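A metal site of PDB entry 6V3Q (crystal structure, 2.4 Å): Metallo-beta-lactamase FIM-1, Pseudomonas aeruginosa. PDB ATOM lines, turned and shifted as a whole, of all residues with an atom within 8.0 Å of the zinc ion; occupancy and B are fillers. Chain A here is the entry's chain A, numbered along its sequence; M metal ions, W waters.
OD2 of Asp 179 lies within hydrogen-bond range of NE2 of His 83 (2.9 Å).
A ring nitrogen (NE2) of His 145 lies close to OD2 of OCS 164 (3.2 Å).
The side-chain amide oxygen (OD1) of Asn 149 sits at hydrogen-bond distance from the backbone NH (N) of His 145 (2.9 Å).
OD1 of OCS 164 lies within salt-bridge range of the side-chain amino group of Lys 86 (3.7 Å).
NE2 of His 206 is in hydrogen-bond range of OD3 of OCS 164, 3.2 Å away.
OD1 of OCS 164 is in hydrogen-bond range of OG of Ser 205 (2.8 Å).
OCS 164 touches the zinc ion (OD2 to ZN, 2.9 Å).
Within 4 Å of the zinc ion: His 81, His 83, His 145 and OCS 164.
The nearest printed residue that does not touch the zinc ion is Asp 85 (4.1 Å).
ND1 of His 83 is bound to the zinc ion, 2.1 Å away.
The zinc ion is bound by NE2 of His 81.
A ring nitrogen (NE2) of His 145 binds the zinc ion (2.3 Å).
The zinc ion has three donor atoms within binding distance.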
ATOM      1  N   TRP A  54      29.711  38.012  25.056  1.00  0.00           N
ATOM      2  CA  TRP A  54      30.595  38.170  23.900  1.00  0.00           C
ATOM      3  C   TRP A  54      32.057  38.213  24.294  1.00  0.00           C
ATOM      4  O   TRP A  54      32.913  37.729  23.543  1.00  0.00           O
ATOM      5  CB  TRP A  54      30.212  39.430  23.126  1.00  0.00           C
ATOM      6  CG  TRP A  54      28.887  39.340  22.446  1.00  0.00           C
ATOM      7  CD1 TRP A  54      27.683  39.735  22.944  1.00  0.00           C
ATOM      8  CD2 TRP A  54      28.626  38.819  21.129  1.00  0.00           C
ATOM      9  NE1 TRP A  54      26.686  39.498  22.024  1.00  0.00           N
ATOM     10  CE2 TRP A  54      27.233  38.933  20.902  1.00  0.00           C
ATOM     11  CE3 TRP A  54      29.425  38.270  20.125  1.00  0.00           C
ATOM     12  CZ2 TRP A  54      26.637  38.522  19.718  1.00  0.00           C
ATOM     13  CZ3 TRP A  54      28.828  37.860  18.941  1.00  0.00           C
ATOM     14  CH2 TRP A  54      27.441  37.991  18.745  1.00  0.00           C
ATOM     15  N   THR A  80      27.517  25.896  23.803  1.00  0.00           N
ATOM     16  CA  THR A  80      26.818  25.170  22.756  1.00  0.00           C
ATOM     17  C   THR A  80      27.609  25.035  21.463  1.00  0.00           C
ATOM     18  O   THR A  80      27.365  24.096  20.698  1.00  0.00           O
ATOM     19  CB  THR A  80      25.454  25.816  22.469  1.00  0.00           C
ATOM     20  OG1 THR A  80      25.647  27.186  22.101  1.00  0.00           O
ATOM     21  CG2 THR A  80      24.580  25.750  23.707  1.00  0.00           C
ATOM     22  N   HIS A  81      28.559  25.934  21.189  1.00  0.00           N
ATOM     23  CA  HIS A  81      29.510  25.741  20.090  1.00  0.00           C
ATOM     24  C   HIS A  81      30.627  26.765  20.241  1.00  0.00           C
ATOM     25  O   HIS A  81      30.581  27.649  21.095  1.00  0.00           O
ATOM     26  CB  HIS A  81      28.840  25.840  18.722  1.00  0.00           C
ATOM     27  CG  HIS A  81      28.354  27.212  18.366  1.00  0.00           C
ATOM     28  ND1 HIS A  81      27.220  27.766  18.931  1.00  0.00           N
ATOM     29  CD2 HIS A  81      28.819  28.117  17.481  1.00  0.00           C
ATOM     30  CE1 HIS A  81      27.019  28.965  18.424  1.00  0.00           C
ATOM     31  NE2 HIS A  81      27.978  29.204  17.547  1.00  0.00           N
ATOM     32  N   ALA A  82      31.642  26.616  19.396  1.00  0.00           N
ATOM     33  CA  ALA A  82      32.890  27.375  19.533  1.00  0.00           C
ATOM     34  C   ALA A  82      32.895  28.591  18.609  1.00  0.00           C
ATOM     35  O   ALA A  82      33.651  28.690  17.649  1.00  0.00           O
ATOM     36  CB  ALA A  82      34.079  26.462  19.264  1.00  0.00           C
ATOM     37  N   HIS A  83      32.003  29.524  18.931  1.00  0.00           N
ATOM     38  CA  HIS A  83      32.021  30.870  18.389  1.00  0.00           C
ATOM     39  C   HIS A  83      32.075  31.858  19.560  1.00  0.00           C
ATOM     40  O   HIS A  83      31.825  31.489  20.708  1.00  0.00           O
ATOM     41  CB  HIS A  83      30.797  31.147  17.497  1.00  0.00           C
ATOM     42  CG  HIS A  83      30.968  30.646  16.096  1.00  0.00           C
ATOM     43  ND1 HIS A  83      29.931  30.636  15.180  1.00  0.00           N
ATOM     44  CD2 HIS A  83      32.046  30.145  15.452  1.00  0.00           C
ATOM     45  CE1 HIS A  83      30.366  30.143  14.028  1.00  0.00           C
ATOM     46  NE2 HIS A  83      31.649  29.843  14.169  1.00  0.00           N
ATOM     47  N   ASP A  84      32.414  33.112  19.259  1.00  0.00           N
ATOM     48  CA  ASP A  84      32.688  34.065  20.337  1.00  0.00           C
ATOM     49  C   ASP A  84      31.442  34.554  21.061  1.00  0.00           C
ATOM     50  O   ASP A  84      31.578  35.145  22.135  1.00  0.00           O
ATOM     51  CB  ASP A  84      33.476  35.265  19.813  1.00  0.00           C
ATOM     52  CG  ASP A  84      32.952  35.788  18.496  1.00  0.00           C
ATOM     53  OD1 ASP A  84      31.760  36.147  18.421  1.00  0.00           O
ATOM     54  OD2 ASP A  84      33.756  35.845  17.531  1.00  0.00           O
ATOM     55  N   ASP A  85      30.239  34.332  20.530  1.00  0.00           N
ATOM     56  CA  ASP A  85      29.055  34.665  21.311  1.00  0.00           C
ATOM     57  C   ASP A  85      28.695  33.583  22.310  1.00  0.00           C
ATOM     58  O   ASP A  85      27.851  33.817  23.187  1.00  0.00           O
ATOM     59  CB  ASP A  85      27.859  34.953  20.392  1.00  0.00           C
ATOM     60  CG  ASP A  85      27.605  33.843  19.399  1.00  0.00           C
ATOM     61  OD1 ASP A  85      28.581  33.167  18.984  1.00  0.00           O
ATOM     62  OD2 ASP A  85      26.439  33.650  19.019  1.00  0.00           O
ATOM     63  N   LYS A  86      29.320  32.407  22.215  1.00  0.00           N
ATOM     64  CA  LYS A  86      29.085  31.315  23.147  1.00  0.00           C
ATOM     65  C   LYS A  86      30.284  31.021  24.034  1.00  0.00           C
ATOM     66  O   LYS A  86      30.087  30.669  25.201  1.00  0.00           O
ATOM     67  CB  LYS A  86      28.712  30.035  22.396  1.00  0.00           C
ATOM     68  CG  LYS A  86      27.523  30.190  21.483  1.00  0.00           C
ATOM     69  CD  LYS A  86      26.430  30.994  22.180  1.00  0.00           C
ATOM     70  CE  LYS A  86      25.225  31.136  21.290  1.00  0.00           C
ATOM     71  NZ  LYS A  86      24.152  31.951  21.919  1.00  0.00           N
ATOM     72  N   HIS A 145      24.268  24.536  12.376  1.00  0.00           N
ATOM     73  CA  HIS A 145      24.871  25.860  12.271  1.00  0.00           C
ATOM     74  C   HIS A 145      26.392  25.769  12.235  1.00  0.00           C
ATOM     75  O   HIS A 145      27.044  26.484  11.462  1.00  0.00           O
ATOM     76  CB  HIS A 145      24.400  26.748  13.421  1.00  0.00           C
ATOM     77  CG  HIS A 145      25.248  27.972  13.621  1.00  0.00           C
ATOM     78  ND1 HIS A 145      25.159  29.079  12.813  1.00  0.00           N
ATOM     79  CD2 HIS A 145      26.197  28.251  14.546  1.00  0.00           C
ATOM     80  CE1 HIS A 145      26.018  29.996  13.227  1.00  0.00           C
ATOM     81  NE2 HIS A 145      26.664  29.517  14.280  1.00  0.00           N
ATOM     82  N   THR A 146      26.965  24.895  13.065  1.00  0.00           N
ATOM     83  CA  THR A 146      28.357  24.506  12.974  1.00  0.00           C
ATOM     84  C   THR A 146      28.423  22.981  13.084  1.00  0.00           C
ATOM     85  O   THR A 146      27.429  22.314  13.371  1.00  0.00           O
ATOM     86  CB  THR A 146      29.222  25.157  14.055  1.00  0.00           C
ATOM     87  OG1 THR A 146      28.732  24.792  15.349  1.00  0.00           O
ATOM     88  CG2 THR A 146      29.194  26.687  13.925  1.00  0.00           C
ATOM     89  N   ASP A 148      29.893  21.419  15.387  1.00  0.00           N
ATOM     90  CA  ASP A 148      30.016  21.035  16.778  1.00  0.00           C
ATOM     91  C   ASP A 148      28.850  21.482  17.659  1.00  0.00           C
ATOM     92  O   ASP A 148      28.900  21.252  18.866  1.00  0.00           O
ATOM     93  CB  ASP A 148      31.313  21.606  17.359  1.00  0.00           C
ATOM     94  CG  ASP A 148      31.379  23.118  17.260  1.00  0.00           C
ATOM     95  OD1 ASP A 148      31.170  23.643  16.148  1.00  0.00           O
ATOM     96  OD2 ASP A 148      31.608  23.784  18.283  1.00  0.00           O
ATOM     97  N   ASN A 149      27.824  22.108  17.088  1.00  0.00           N
ATOM     98  CA  ASN A 149      26.773  22.694  17.924  1.00  0.00           C
ATOM     99  C   ASN A 149      26.024  21.623  18.698  1.00  0.00           C
ATOM    100  O   ASN A 149      25.727  20.539  18.183  1.00  0.00           O
ATOM    101  CB  ASN A 149      25.798  23.524  17.086  1.00  0.00           C
ATOM    102  CG  ASN A 149      25.215  22.767  15.892  1.00  0.00           C
ATOM    103  OD1 ASN A 149      24.729  23.384  14.951  1.00  0.00           O
ATOM    104  ND2 ASN A 149      25.255  21.441  15.930  1.00  0.00           N
ATOM    105  N   GLY A 163      20.301  27.496  20.896  1.00  0.00           N
ATOM    106  CA  GLY A 163      21.496  28.175  20.437  1.00  0.00           C
ATOM    107  C   GLY A 163      21.339  28.664  19.015  1.00  0.00           C
ATOM    108  O   GLY A 163      20.227  28.988  18.583  1.00  0.00           O
ATOM    109  N   OCS A 164      22.438  28.724  18.282  1.00  0.00           N
ATOM    110  CA  OCS A 164      22.393  29.172  16.863  1.00  0.00           C
ATOM    111  CB  OCS A 164      23.795  29.571  16.410  1.00  0.00           C
ATOM    112  SG  OCS A 164      24.052  31.162  16.832  1.00  0.00           S
ATOM    113  C   OCS A 164      21.840  28.135  15.929  1.00  0.00           C
ATOM    114  O   OCS A 164      21.636  28.406  14.747  1.00  0.00           O
ATOM    115  OD1 OCS A 164      24.354  31.240  18.272  1.00  0.00           O
ATOM    116  OD2 OCS A 164      25.190  31.698  16.060  1.00  0.00           O
ATOM    117  OD3 OCS A 164      22.826  31.937  16.540  1.00  0.00           O
ATOM    118  N   LEU A 165      21.583  26.942  16.448  1.00  0.00           N
ATOM    119  CA  LEU A 165      20.982  25.872  15.652  1.00  0.00           C
ATOM    120  C   LEU A 165      19.542  26.235  15.305  1.00  0.00           C
ATOM    121  O   LEU A 165      19.025  25.833  14.266  1.00  0.00           O
ATOM    122  CB  LEU A 165      21.035  24.532  16.397  1.00  0.00           C
ATOM    123  CG  LEU A 165      20.461  23.336  15.639  1.00  0.00           C
ATOM    124  CD1 LEU A 165      21.290  23.011  14.408  1.00  0.00           C
ATOM    125  CD2 LEU A 165      20.357  22.109  16.543  1.00  0.00           C
ATOM    126  N   ASN A 176      24.597  33.507   9.146  1.00  0.00           N
ATOM    127  CA  ASN A 176      25.983  33.176   8.829  1.00  0.00           C
ATOM    128  C   ASN A 176      26.096  31.680   8.559  1.00  0.00           C
ATOM    129  O   ASN A 176      25.946  30.865   9.473  1.00  0.00           O
ATOM    130  CB  ASN A 176      26.903  33.591   9.967  1.00  0.00           C
ATOM    131  CG  ASN A 176      28.326  33.106   9.779  1.00  0.00           C
ATOM    132  OD1 ASN A 176      28.903  33.235   8.703  1.00  0.00           O
ATOM    133  ND2 ASN A 176      28.885  32.522  10.827  1.00  0.00           N
ATOM    134  N   ASP A 179      30.349  28.273   8.346  1.00  0.00           N
ATOM    135  CA  ASP A 179      30.776  27.031   8.975  1.00  0.00           C
ATOM    136  C   ASP A 179      29.657  26.006   9.055  1.00  0.00           C
ATOM    137  O   ASP A 179      29.786  25.020   9.801  1.00  0.00           O
ATOM    138  CB  ASP A 179      31.323  27.324  10.374  1.00  0.00           C
ATOM    139  CG  ASP A 179      32.249  28.523  10.406  1.00  0.00           C
ATOM    140  OD1 ASP A 179      33.076  28.673   9.481  1.00  0.00           O
ATOM    141  OD2 ASP A 179      32.160  29.320  11.365  1.00  0.00           O
ATOM    142  N   SER A 205      19.353  31.797  19.946  1.00  0.00           N
ATOM    143  CA  SER A 205      20.468  32.615  20.414  1.00  0.00           C
ATOM    144  C   SER A 205      20.177  34.100  20.284  1.00  0.00           C
ATOM    145  O   SER A 205      20.704  34.891  21.068  1.00  0.00           O
ATOM    146  CB  SER A 205      21.741  32.258  19.652  1.00  0.00           C
ATOM    147  OG  SER A 205      22.373  31.133  20.218  1.00  0.00           O
ATOM    148  N   HIS A 206      19.364  34.498  19.308  1.00  0.00           N
ATOM    149  CA  HIS A 206      19.057  35.891  19.056  1.00  0.00           C
ATOM    150  C   HIS A 206      17.561  36.130  19.167  1.00  0.00           C
ATOM    151  O   HIS A 206      16.759  35.327  18.677  1.00  0.00           O
ATOM    152  CB  HIS A 206      19.547  36.321  17.670  1.00  0.00           C
ATOM    153  CG  HIS A 206      20.960  35.927  17.398  1.00  0.00           C
ATOM    154  ND1 HIS A 206      21.990  36.235  18.252  1.00  0.00           N
ATOM    155  CD2 HIS A 206      21.513  35.256  16.354  1.00  0.00           C
ATOM    156  CE1 HIS A 206      23.129  35.765  17.757  1.00  0.00           C
ATOM    157  NE2 HIS A 206      22.865  35.174  16.607  1.00  0.00           N
HETATM  158 ZN    ZN M   1      27.891  30.606  15.830  1.00  0.00          ZN
HETATM  159  O   HOH W   1      27.419  32.954  14.232  1.00  0.00           O
